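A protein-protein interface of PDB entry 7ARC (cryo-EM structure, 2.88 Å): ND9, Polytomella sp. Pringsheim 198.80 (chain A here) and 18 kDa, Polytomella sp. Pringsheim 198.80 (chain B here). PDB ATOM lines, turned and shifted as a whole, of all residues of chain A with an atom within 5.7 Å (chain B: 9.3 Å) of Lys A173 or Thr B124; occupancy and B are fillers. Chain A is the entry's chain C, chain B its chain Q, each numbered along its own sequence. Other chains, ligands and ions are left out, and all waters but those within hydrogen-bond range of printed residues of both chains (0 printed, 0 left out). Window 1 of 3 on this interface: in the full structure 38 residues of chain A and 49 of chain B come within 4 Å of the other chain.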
ATOM      1  N   ASP A  91      -3.334 -21.750 -10.093  1.00  0.00           N
ATOM      2  CA  ASP A  91      -3.509 -21.735 -11.539  1.00  0.00           C
ATOM      3  C   ASP A  91      -4.896 -21.203 -11.879  1.00  0.00           C
ATOM      4  O   ASP A  91      -5.904 -21.731 -11.399  1.00  0.00           O
ATOM      5  CB  ASP A  91      -3.310 -23.142 -12.105  1.00  0.00           C
ATOM      6  CG  ASP A  91      -3.579 -23.230 -13.598  1.00  0.00           C
ATOM      7  OD1 ASP A  91      -3.556 -24.357 -14.130  1.00  0.00           O
ATOM      8  OD2 ASP A  91      -3.778 -22.189 -14.253  1.00  0.00           O
ATOM      9  N   TYR A  92      -4.943 -20.154 -12.702  1.00  0.00           N
ATOM     10  CA  TYR A  92      -6.187 -19.571 -13.203  1.00  0.00           C
ATOM     11  C   TYR A  92      -6.147 -19.639 -14.722  1.00  0.00           C
ATOM     12  O   TYR A  92      -5.688 -18.694 -15.380  1.00  0.00           O
ATOM     13  CB  TYR A  92      -6.365 -18.131 -12.738  1.00  0.00           C
ATOM     14  CG  TYR A  92      -6.606 -17.956 -11.262  1.00  0.00           C
ATOM     15  CD1 TYR A  92      -7.871 -18.126 -10.721  1.00  0.00           C
ATOM     16  CD2 TYR A  92      -5.578 -17.581 -10.414  1.00  0.00           C
ATOM     17  CE1 TYR A  92      -8.097 -17.955  -9.374  1.00  0.00           C
ATOM     18  CE2 TYR A  92      -5.796 -17.406  -9.069  1.00  0.00           C
ATOM     19  CZ  TYR A  92      -7.054 -17.593  -8.552  1.00  0.00           C
ATOM     20  OH  TYR A  92      -7.269 -17.417  -7.208  1.00  0.00           O
ATOM     21  N   PRO A  93      -6.615 -20.733 -15.326  1.00  0.00           N
ATOM     22  CA  PRO A  93      -6.530 -20.851 -16.790  1.00  0.00           C
ATOM     23  C   PRO A  93      -7.323 -19.800 -17.549  1.00  0.00           C
ATOM     24  O   PRO A  93      -6.993 -19.521 -18.707  1.00  0.00           O
ATOM     25  CB  PRO A  93      -7.066 -22.263 -17.055  1.00  0.00           C
ATOM     26  CG  PRO A  93      -7.923 -22.559 -15.872  1.00  0.00           C
ATOM     27  CD  PRO A  93      -7.212 -21.930 -14.718  1.00  0.00           C
ATOM     28  N   ARG A  98      -1.582 -16.844 -15.994  1.00  0.00           N
ATOM     29  CA  ARG A  98      -2.297 -17.931 -15.331  1.00  0.00           C
ATOM     30  C   ARG A  98      -1.958 -18.022 -13.847  1.00  0.00           C
ATOM     31  O   ARG A  98      -2.855 -18.185 -13.013  1.00  0.00           O
ATOM     32  CB  ARG A  98      -1.980 -19.254 -16.025  1.00  0.00           C
ATOM     33  CG  ARG A  98      -2.869 -19.553 -17.212  1.00  0.00           C
ATOM     34  CD  ARG A  98      -2.526 -20.885 -17.857  1.00  0.00           C
ATOM     35  NE  ARG A  98      -2.563 -21.996 -16.915  1.00  0.00           N
ATOM     36  CZ  ARG A  98      -2.246 -23.245 -17.224  1.00  0.00           C
ATOM     37  NH1 ARG A  98      -1.834 -23.574 -18.436  1.00  0.00           N
ATOM     38  NH2 ARG A  98      -2.356 -24.190 -16.296  1.00  0.00           N
ATOM     39  N   PRO A 170       1.772 -31.487 -12.150  1.00  0.00           N
ATOM     40  CA  PRO A 170       0.469 -32.094 -11.839  1.00  0.00           C
ATOM     41  C   PRO A 170      -0.606 -31.117 -11.392  1.00  0.00           C
ATOM     42  O   PRO A 170      -1.778 -31.320 -11.728  1.00  0.00           O
ATOM     43  CB  PRO A 170       0.828 -33.100 -10.741  1.00  0.00           C
ATOM     44  CG  PRO A 170       1.996 -32.491 -10.067  1.00  0.00           C
ATOM     45  CD  PRO A 170       2.800 -31.865 -11.168  1.00  0.00           C
ATOM     46  N   LEU A 171      -0.262 -30.073 -10.643  1.00  0.00           N
ATOM     47  CA  LEU A 171      -1.292 -29.199 -10.087  1.00  0.00           C
ATOM     48  C   LEU A 171      -1.832 -28.186 -11.086  1.00  0.00           C
ATOM     49  O   LEU A 171      -2.709 -27.396 -10.725  1.00  0.00           O
ATOM     50  CB  LEU A 171      -0.763 -28.466  -8.853  1.00  0.00           C
ATOM     51  CG  LEU A 171      -0.807 -29.256  -7.547  1.00  0.00           C
ATOM     52  CD1 LEU A 171      -0.093 -28.512  -6.444  1.00  0.00           C
ATOM     53  CD2 LEU A 171      -2.242 -29.525  -7.155  1.00  0.00           C
ATOM     54  N   ARG A 172      -1.332 -28.182 -12.316  1.00  0.00           N
ATOM     55  CA  ARG A 172      -1.948 -27.397 -13.374  1.00  0.00           C
ATOM     56  C   ARG A 172      -3.357 -27.911 -13.653  1.00  0.00           C
ATOM     57  O   ARG A 172      -3.591 -29.121 -13.704  1.00  0.00           O
ATOM     58  CB  ARG A 172      -1.093 -27.470 -14.634  1.00  0.00           C
ATOM     59  CG  ARG A 172       0.055 -26.489 -14.654  1.00  0.00           C
ATOM     60  CD  ARG A 172       0.682 -26.417 -16.027  1.00  0.00           C
ATOM     61  NE  ARG A 172       2.001 -25.800 -15.989  1.00  0.00           N
ATOM     62  CZ  ARG A 172       2.623 -25.301 -17.046  1.00  0.00           C
ATOM     63  NH1 ARG A 172       2.079 -25.339 -18.250  1.00  0.00           N
ATOM     64  NH2 ARG A 172       3.825 -24.755 -16.893  1.00  0.00           N
ATOM     65  N   LYS A 173      -4.303 -26.984 -13.829  1.00  0.00           N
ATOM     66  CA  LYS A 173      -5.700 -27.368 -14.018  1.00  0.00           C
ATOM     67  C   LYS A 173      -5.929 -28.191 -15.277  1.00  0.00           C
ATOM     68  O   LYS A 173      -6.949 -28.881 -15.372  1.00  0.00           O
ATOM     69  CB  LYS A 173      -6.596 -26.131 -14.063  1.00  0.00           C
ATOM     70  CG  LYS A 173      -6.610 -25.304 -12.799  1.00  0.00           C
ATOM     71  CD  LYS A 173      -7.275 -26.075 -11.677  1.00  0.00           C
ATOM     72  CE  LYS A 173      -7.379 -25.243 -10.415  1.00  0.00           C
ATOM     73  NZ  LYS A 173      -7.997 -26.016  -9.303  1.00  0.00           N
ATOM     74  N   ASP A 174      -5.014 -28.147 -16.237  1.00  0.00           N
ATOM     75  CA  ASP A 174      -5.142 -28.936 -17.452  1.00  0.00           C
ATOM     76  C   ASP A 174      -4.550 -30.335 -17.327  1.00  0.00           C
ATOM     77  O   ASP A 174      -4.650 -31.121 -18.273  1.00  0.00           O
ATOM     78  CB  ASP A 174      -4.497 -28.191 -18.624  1.00  0.00           C
ATOM     79  CG  ASP A 174      -3.006 -27.974 -18.435  1.00  0.00           C
ATOM     80  OD1 ASP A 174      -2.461 -28.360 -17.382  1.00  0.00           O
ATOM     81  OD2 ASP A 174      -2.371 -27.414 -19.346  1.00  0.00           O
ATOM     82  N   PHE A 175      -3.934 -30.658 -16.198  1.00  0.00           N
ATOM     83  CA  PHE A 175      -3.370 -31.987 -15.991  1.00  0.00           C
ATOM     84  C   PHE A 175      -4.453 -32.945 -15.505  1.00  0.00           C
ATOM     85  O   PHE A 175      -5.205 -32.603 -14.588  1.00  0.00           O
ATOM     86  CB  PHE A 175      -2.228 -31.926 -14.983  1.00  0.00           C
ATOM     87  CG  PHE A 175      -1.388 -33.168 -14.940  1.00  0.00           C
ATOM     88  CD1 PHE A 175      -0.396 -33.378 -15.875  1.00  0.00           C
ATOM     89  CD2 PHE A 175      -1.589 -34.120 -13.960  1.00  0.00           C
ATOM     90  CE1 PHE A 175       0.375 -34.515 -15.835  1.00  0.00           C
ATOM     91  CE2 PHE A 175      -0.820 -35.260 -13.918  1.00  0.00           C
ATOM     92  CZ  PHE A 175       0.162 -35.457 -14.855  1.00  0.00           C
ATOM     93  N   VAL B  57       3.399 -32.770 -21.070  1.00  0.00           N
ATOM     94  CA  VAL B  57       2.449 -33.866 -21.224  1.00  0.00           C
ATOM     95  C   VAL B  57       2.756 -34.589 -22.531  1.00  0.00           C
ATOM     96  O   VAL B  57       3.496 -34.051 -23.369  1.00  0.00           O
ATOM     97  CB  VAL B  57       1.006 -33.346 -21.194  1.00  0.00           C
ATOM     98  CG1 VAL B  57       0.631 -32.939 -19.784  1.00  0.00           C
ATOM     99  CG2 VAL B  57       0.848 -32.183 -22.143  1.00  0.00           C
ATOM    100  N   PRO B  91     -17.828 -18.713 -14.430  1.00  0.00           N
ATOM    101  CA  PRO B  91     -17.382 -19.183 -15.747  1.00  0.00           C
ATOM    102  C   PRO B  91     -18.244 -20.330 -16.254  1.00  0.00           C
ATOM    103  O   PRO B  91     -18.511 -21.294 -15.536  1.00  0.00           O
ATOM    104  CB  PRO B  91     -15.943 -19.635 -15.482  1.00  0.00           C
ATOM    105  CG  PRO B  91     -15.520 -18.823 -14.310  1.00  0.00           C
ATOM    106  CD  PRO B  91     -16.739 -18.772 -13.443  1.00  0.00           C
ATOM    107  N   GLN B  92     -18.684 -20.213 -17.506  1.00  0.00           N
ATOM    108  CA  GLN B  92     -19.623 -21.161 -18.083  1.00  0.00           C
ATOM    109  C   GLN B  92     -19.197 -21.775 -19.407  1.00  0.00           C
ATOM    110  O   GLN B  92     -19.925 -22.624 -19.929  1.00  0.00           O
ATOM    111  CB  GLN B  92     -20.998 -20.519 -18.245  1.00  0.00           C
ATOM    112  CG  GLN B  92     -21.628 -20.191 -16.926  1.00  0.00           C
ATOM    113  CD  GLN B  92     -22.957 -19.548 -17.102  1.00  0.00           C
ATOM    114  OE1 GLN B  92     -23.374 -19.284 -18.225  1.00  0.00           O
ATOM    115  NE2 GLN B  92     -23.665 -19.340 -16.005  1.00  0.00           N
ATOM    116  N   TRP B  93     -18.058 -21.387 -19.962  1.00  0.00           N
ATOM    117  CA  TRP B  93     -17.595 -21.934 -21.227  1.00  0.00           C
ATOM    118  C   TRP B  93     -16.625 -23.059 -20.907  1.00  0.00           C
ATOM    119  O   TRP B  93     -15.621 -22.839 -20.222  1.00  0.00           O
ATOM    120  CB  TRP B  93     -16.917 -20.854 -22.068  1.00  0.00           C
ATOM    121  CG  TRP B  93     -17.875 -19.909 -22.720  1.00  0.00           C
ATOM    122  CD1 TRP B  93     -18.393 -18.773 -22.178  1.00  0.00           C
ATOM    123  CD2 TRP B  93     -18.423 -20.007 -24.039  1.00  0.00           C
ATOM    124  NE1 TRP B  93     -19.233 -18.160 -23.070  1.00  0.00           N
ATOM    125  CE2 TRP B  93     -19.270 -18.898 -24.222  1.00  0.00           C
ATOM    126  CE3 TRP B  93     -18.283 -20.925 -25.080  1.00  0.00           C
ATOM    127  CZ2 TRP B  93     -19.970 -18.683 -25.404  1.00  0.00           C
ATOM    128  CZ3 TRP B  93     -18.980 -20.710 -26.250  1.00  0.00           C
ATOM    129  CH2 TRP B  93     -19.812 -19.599 -26.403  1.00  0.00           C
ATOM    130  N   LYS B  94     -16.924 -24.257 -21.393  1.00  0.00           N
ATOM    131  CA  LYS B  94     -16.090 -25.417 -21.140  1.00  0.00           C
ATOM    132  C   LYS B  94     -15.304 -25.814 -22.380  1.00  0.00           C
ATOM    133  O   LYS B  94     -15.779 -25.685 -23.510  1.00  0.00           O
ATOM    134  CB  LYS B  94     -16.929 -26.612 -20.683  1.00  0.00           C
ATOM    135  CG  LYS B  94     -17.587 -26.442 -19.333  1.00  0.00           C
ATOM    136  CD  LYS B  94     -18.242 -27.736 -18.889  1.00  0.00           C
ATOM    137  CE  LYS B  94     -19.510 -28.012 -19.668  1.00  0.00           C
ATOM    138  NZ  LYS B  94     -20.219 -29.222 -19.169  1.00  0.00           N
ATOM    139  N   ILE B  95     -14.089 -26.292 -22.145  1.00  0.00           N
ATOM    140  CA  ILE B  95     -13.349 -27.080 -23.120  1.00  0.00           C
ATOM    141  C   ILE B  95     -13.627 -28.552 -22.857  1.00  0.00           C
ATOM    142  O   ILE B  95     -13.375 -29.047 -21.756  1.00  0.00           O
ATOM    143  CB  ILE B  95     -11.845 -26.783 -23.044  1.00  0.00           C
ATOM    144  CG1 ILE B  95     -11.550 -25.333 -23.431  1.00  0.00           C
ATOM    145  CG2 ILE B  95     -11.040 -27.800 -23.826  1.00  0.00           C
ATOM    146  CD1 ILE B  95     -10.134 -24.916 -23.139  1.00  0.00           C
ATOM    147  N   VAL B  96     -14.154 -29.251 -23.855  1.00  0.00           N
ATOM    148  CA  VAL B  96     -14.450 -30.671 -23.731  1.00  0.00           C
ATOM    149  C   VAL B  96     -13.775 -31.402 -24.879  1.00  0.00           C
ATOM    150  O   VAL B  96     -13.677 -30.876 -25.994  1.00  0.00           O
ATOM    151  CB  VAL B  96     -15.964 -30.965 -23.709  1.00  0.00           C
ATOM    152  CG1 VAL B  96     -16.591 -30.386 -22.457  1.00  0.00           C
ATOM    153  CG2 VAL B  96     -16.634 -30.429 -24.954  1.00  0.00           C
ATOM    154  N   PHE B  97     -13.295 -32.603 -24.602  1.00  0.00           N
ATOM    155  CA  PHE B  97     -12.684 -33.458 -25.603  1.00  0.00           C
ATOM    156  C   PHE B  97     -13.677 -34.522 -26.051  1.00  0.00           C
ATOM    157  O   PHE B  97     -14.641 -34.839 -25.350  1.00  0.00           O
ATOM    158  CB  PHE B  97     -11.409 -34.093 -25.049  1.00  0.00           C
ATOM    159  CG  PHE B  97     -10.428 -33.091 -24.520  1.00  0.00           C
ATOM    160  CD1 PHE B  97      -9.464 -32.541 -25.344  1.00  0.00           C
ATOM    161  CD2 PHE B  97     -10.477 -32.688 -23.197  1.00  0.00           C
ATOM    162  CE1 PHE B  97      -8.570 -31.614 -24.859  1.00  0.00           C
ATOM    163  CE2 PHE B  97      -9.583 -31.765 -22.710  1.00  0.00           C
ATOM    164  CZ  PHE B  97      -8.629 -31.228 -23.540  1.00  0.00           C
ATOM    165  N   LEU B 117      -7.976 -37.820 -20.598  1.00  0.00           N
ATOM    166  CA  LEU B 117      -8.659 -36.533 -20.577  1.00  0.00           C
ATOM    167  C   LEU B 117     -10.170 -36.666 -20.471  1.00  0.00           C
ATOM    168  O   LEU B 117     -10.896 -35.807 -20.986  1.00  0.00           O
ATOM    169  CB  LEU B 117      -8.299 -35.725 -21.822  1.00  0.00           C
ATOM    170  CG  LEU B 117      -6.826 -35.533 -22.155  1.00  0.00           C
ATOM    171  CD1 LEU B 117      -6.693 -35.088 -23.596  1.00  0.00           C
ATOM    172  CD2 LEU B 117      -6.201 -34.520 -21.216  1.00  0.00           C
ATOM    173  N   GLU B 118     -10.665 -37.723 -19.829  1.00  0.00           N
ATOM    174  CA  GLU B 118     -12.101 -37.976 -19.830  1.00  0.00           C
ATOM    175  C   GLU B 118     -12.867 -36.871 -19.113  1.00  0.00           C
ATOM    176  O   GLU B 118     -13.842 -36.330 -19.648  1.00  0.00           O
ATOM    177  CB  GLU B 118     -12.400 -39.325 -19.186  1.00  0.00           C
ATOM    178  CG  GLU B 118     -13.870 -39.666 -19.225  1.00  0.00           C
ATOM    179  CD  GLU B 118     -14.174 -41.014 -18.630  1.00  0.00           C
ATOM    180  OE1 GLU B 118     -13.235 -41.688 -18.166  1.00  0.00           O
ATOM    181  OE2 GLU B 118     -15.363 -41.384 -18.605  1.00  0.00           O
ATOM    182  N   ASN B 119     -12.451 -36.526 -17.895  1.00  0.00           N
ATOM    183  CA  ASN B 119     -13.238 -35.638 -17.054  1.00  0.00           C
ATOM    184  C   ASN B 119     -12.566 -34.309 -16.740  1.00  0.00           C
ATOM    185  O   ASN B 119     -13.165 -33.488 -16.040  1.00  0.00           O
ATOM    186  CB  ASN B 119     -13.630 -36.353 -15.749  1.00  0.00           C
ATOM    187  CG  ASN B 119     -12.441 -36.670 -14.857  1.00  0.00           C
ATOM    188  OD1 ASN B 119     -11.565 -35.838 -14.625  1.00  0.00           O
ATOM    189  ND2 ASN B 119     -12.408 -37.895 -14.350  1.00  0.00           N
ATOM    190  N   VAL B 120     -11.341 -34.076 -17.211  1.00  0.00           N
ATOM    191  CA  VAL B 120     -10.635 -32.851 -16.844  1.00  0.00           C
ATOM    192  C   VAL B 120     -11.344 -31.629 -17.418  1.00  0.00           C
ATOM    193  O   VAL B 120     -11.571 -30.635 -16.715  1.00  0.00           O
ATOM    194  CB  VAL B 120      -9.158 -32.927 -17.279  1.00  0.00           C
ATOM    195  CG1 VAL B 120      -9.031 -33.210 -18.766  1.00  0.00           C
ATOM    196  CG2 VAL B 120      -8.437 -31.641 -16.924  1.00  0.00           C
ATOM    197  N   GLY B 121     -11.722 -31.692 -18.695  1.00  0.00           N
ATOM    198  CA  GLY B 121     -12.315 -30.535 -19.343  1.00  0.00           C
ATOM    199  C   GLY B 121     -13.672 -30.167 -18.775  1.00  0.00           C
ATOM    200  O   GLY B 121     -13.960 -28.993 -18.532  1.00  0.00           O
ATOM    201  N   ARG B 122     -14.532 -31.166 -18.574  1.00  0.00           N
ATOM    202  CA  ARG B 122     -15.845 -30.910 -17.994  1.00  0.00           C
ATOM    203  C   ARG B 122     -15.724 -30.367 -16.574  1.00  0.00           C
ATOM    204  O   ARG B 122     -16.472 -29.464 -16.181  1.00  0.00           O
ATOM    205  CB  ARG B 122     -16.682 -32.192 -18.025  1.00  0.00           C
ATOM    206  CG  ARG B 122     -16.087 -33.306 -17.185  1.00  0.00           C
ATOM    207  CD  ARG B 122     -16.866 -34.607 -17.188  1.00  0.00           C
ATOM    208  NE  ARG B 122     -18.157 -34.473 -16.529  1.00  0.00           N
ATOM    209  CZ  ARG B 122     -19.135 -35.362 -16.617  1.00  0.00           C
ATOM    210  NH1 ARG B 122     -18.972 -36.503 -17.264  1.00  0.00           N
ATOM    211  NH2 ARG B 122     -20.294 -35.113 -16.017  1.00  0.00           N
ATOM    212  N   SER B 123     -14.795 -30.908 -15.788  1.00  0.00           N
ATOM    213  CA  SER B 123     -14.753 -30.615 -14.362  1.00  0.00           C
ATOM    214  C   SER B 123     -14.074 -29.281 -14.061  1.00  0.00           C
ATOM    215  O   SER B 123     -14.582 -28.501 -13.250  1.00  0.00           O
ATOM    216  CB  SER B 123     -14.069 -31.757 -13.613  1.00  0.00           C
ATOM    217  OG  SER B 123     -12.669 -31.577 -13.561  1.00  0.00           O
ATOM    218  N   THR B 124     -12.932 -28.993 -14.694  1.00  0.00           N
ATOM    219  CA  THR B 124     -12.108 -27.862 -14.286  1.00  0.00           C
ATOM    220  C   THR B 124     -11.911 -26.777 -15.335  1.00  0.00           C
ATOM    221  O   THR B 124     -11.623 -25.637 -14.956  1.00  0.00           O
ATOM    222  CB  THR B 124     -10.720 -28.338 -13.826  1.00  0.00           C
ATOM    223  OG1 THR B 124     -10.050 -28.998 -14.906  1.00  0.00           O
ATOM    224  CG2 THR B 124     -10.830 -29.271 -12.632  1.00  0.00           C
ATOM    225  N   LEU B 125     -12.045 -27.078 -16.622  1.00  0.00           N
ATOM    226  CA  LEU B 125     -11.752 -26.090 -17.661  1.00  0.00           C
ATOM    227  C   LEU B 125     -12.989 -25.226 -17.874  1.00  0.00           C
ATOM    228  O   LEU B 125     -13.813 -25.479 -18.751  1.00  0.00           O
ATOM    229  CB  LEU B 125     -11.320 -26.772 -18.955  1.00  0.00           C
ATOM    230  CG  LEU B 125      -9.861 -27.212 -19.130  1.00  0.00           C
ATOM    231  CD1 LEU B 125      -8.928 -26.013 -19.123  1.00  0.00           C
ATOM    232  CD2 LEU B 125      -9.435 -28.226 -18.088  1.00  0.00           C
ATOM    233  N   LEU B 126     -13.112 -24.185 -17.052  1.00  0.00           N
ATOM    234  CA  LEU B 126     -14.218 -23.237 -17.103  1.00  0.00           C
ATOM    235  C   LEU B 126     -13.671 -21.850 -17.405  1.00  0.00           C
ATOM    236  O   LEU B 126     -12.691 -21.421 -16.787  1.00  0.00           O
ATOM    237  CB  LEU B 126     -15.003 -23.220 -15.787  1.00  0.00           C
ATOM    238  CG  LEU B 126     -16.088 -24.276 -15.546  1.00  0.00           C
ATOM    239  CD1 LEU B 126     -17.215 -24.124 -16.556  1.00  0.00           C
ATOM    240  CD2 LEU B 126     -15.542 -25.694 -15.561  1.00  0.00           C
ATOM    241  N   PHE B 127     -14.308 -21.147 -18.339  1.00  0.00           N
ATOM    242  CA  PHE B 127     -13.845 -19.839 -18.779  1.00  0.00           C
ATOM    243  C   PHE B 127     -15.009 -18.865 -18.851  1.00  0.00           C
ATOM    244  O   PHE B 127     -16.142 -19.241 -19.160  1.00  0.00           O
ATOM    245  CB  PHE B 127     -13.166 -19.912 -20.151  1.00  0.00           C
ATOM    246  CG  PHE B 127     -12.003 -20.854 -20.202  1.00  0.00           C
ATOM    247  CD1 PHE B 127     -12.194 -22.197 -20.456  1.00  0.00           C
ATOM    248  CD2 PHE B 127     -10.716 -20.393 -20.008  1.00  0.00           C
ATOM    249  CE1 PHE B 127     -11.130 -23.057 -20.501  1.00  0.00           C
ATOM    250  CE2 PHE B 127      -9.649 -21.254 -20.057  1.00  0.00           C
ATOM    251  CZ  PHE B 127      -9.856 -22.587 -20.304  1.00  0.00           C
ATOM    252  N   PHE B 136      -6.756 -20.109 -24.742  1.00  0.00           N
ATOM    253  CA  PHE B 136      -6.145 -21.232 -24.036  1.00  0.00           C
ATOM    254  C   PHE B 136      -5.854 -22.384 -24.994  1.00  0.00           C
ATOM    255  O   PHE B 136      -4.759 -22.965 -24.980  1.00  0.00           O
ATOM    256  CB  PHE B 136      -7.073 -21.675 -22.903  1.00  0.00           C
ATOM    257  CG  PHE B 136      -6.473 -22.688 -21.974  1.00  0.00           C
ATOM    258  CD1 PHE B 136      -5.682 -22.285 -20.913  1.00  0.00           C
ATOM    259  CD2 PHE B 136      -6.713 -24.038 -22.146  1.00  0.00           C
ATOM    260  CE1 PHE B 136      -5.135 -23.209 -20.051  1.00  0.00           C
ATOM    261  CE2 PHE B 136      -6.167 -24.966 -21.287  1.00  0.00           C
ATOM    262  CZ  PHE B 136      -5.377 -24.551 -20.239  1.00  0.00           C
ATOM    263  N   HIS B 140      -2.109 -23.796 -26.097  1.00  0.00           N
ATOM    264  CA  HIS B 140      -1.647 -25.171 -25.948  1.00  0.00           C
ATOM    265  C   HIS B 140      -1.527 -25.923 -27.266  1.00  0.00           C
ATOM    266  O   HIS B 140      -0.872 -26.967 -27.306  1.00  0.00           O
ATOM    267  CB  HIS B 140      -2.563 -25.917 -24.985  1.00  0.00           C
ATOM    268  CG  HIS B 140      -2.319 -25.556 -23.556  1.00  0.00           C
ATOM    269  ND1 HIS B 140      -1.540 -26.322 -22.718  1.00  0.00           N
ATOM    270  CD2 HIS B 140      -2.727 -24.493 -22.826  1.00  0.00           C
ATOM    271  CE1 HIS B 140      -1.487 -25.749 -21.530  1.00  0.00           C
ATOM    272  NE2 HIS B 140      -2.203 -24.641 -21.567  1.00  0.00           N
ATOM    273  N   TRP B 142      -4.265 -27.024 -29.137  1.00  0.00           N
ATOM    274  CA  TRP B 142      -5.444 -27.821 -29.441  1.00  0.00           C
ATOM    275  C   TRP B 142      -6.242 -27.172 -30.562  1.00  0.00           C
ATOM    276  O   TRP B 142      -6.512 -25.968 -30.526  1.00  0.00           O
ATOM    277  CB  TRP B 142      -6.325 -27.973 -28.206  1.00  0.00           C
ATOM    278  CG  TRP B 142      -5.896 -29.026 -27.247  1.00  0.00           C
ATOM    279  CD1 TRP B 142      -5.645 -30.332 -27.529  1.00  0.00           C
ATOM    280  CD2 TRP B 142      -5.697 -28.872 -25.840  1.00  0.00           C
ATOM    281  NE1 TRP B 142      -5.288 -31.002 -26.388  1.00  0.00           N
ATOM    282  CE2 TRP B 142      -5.312 -30.127 -25.336  1.00  0.00           C
ATOM    283  CE3 TRP B 142      -5.798 -27.793 -24.960  1.00  0.00           C
ATOM    284  CZ2 TRP B 142      -5.028 -30.334 -23.990  1.00  0.00           C
ATOM    285  CZ3 TRP B 142      -5.518 -28.000 -23.625  1.00  0.00           C
ATOM    286  CH2 TRP B 142      -5.136 -29.260 -23.152  1.00  0.00           C
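Among the printed residues, 8 pairs touch across the chains.
Among the printed residues, merely in contact across the chains: Pro A93 with Phe B127 (3.4 Å), Pro A93 with Phe B136 (3.7 Å), Arg A98 with Phe B136 (3.7 Å), Lys A173 with Val B120 (3.5 Å), Lys A173 with Leu B125 (3.7 Å) and Asp A174 with His B140 (2.9 Å).
OD1 of Asp A91 lies within salt-bridge range of NH2 of Arg A98, at 2.5 Å.
N of Phe B127 lies within hydrogen-bond range of O of Trp B93 (2.9 Å).
The backbone NH (N) of Gln B92 is in hydrogen-bond range of the backbone carbonyl oxygen (O) of Phe B127, 3.2 Å away.
The backbone carbonyl oxygen (O) of Val B120 sits at hydrogen-bond distance from the side-chain hydroxyl (OG) of Ser B123 (3.5 Å).
O of Val B120 sits at hydrogen-bond distance from OG1 of Thr B124, at 2.9 Å.
OD1 of Asp A91 lies within hydrogen-bond range of N of Lys A173.
The side-chain hydroxyl of Thr B124 sits at hydrogen-bond distance from the backbone carbonyl oxygen of Lys A173 (3.1 Å).
A ring nitrogen (NE2) of His B140 is in hydrogen-bond range of the guanidinium group of Arg A98 (3.3 Å).
Of the printed residues of chain B, Pro A93 touches Phe B127 and Phe B136.
Lys A173 touches just these residues of chain B: Val B120, Thr B124 and Leu B125.
Of the printed residues of chain A, Leu B125 touches Lys A173 (3.7 Å).
The nearest residue of chain B that does not touch Lys A173 is Phe B136 (6.2 Å).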
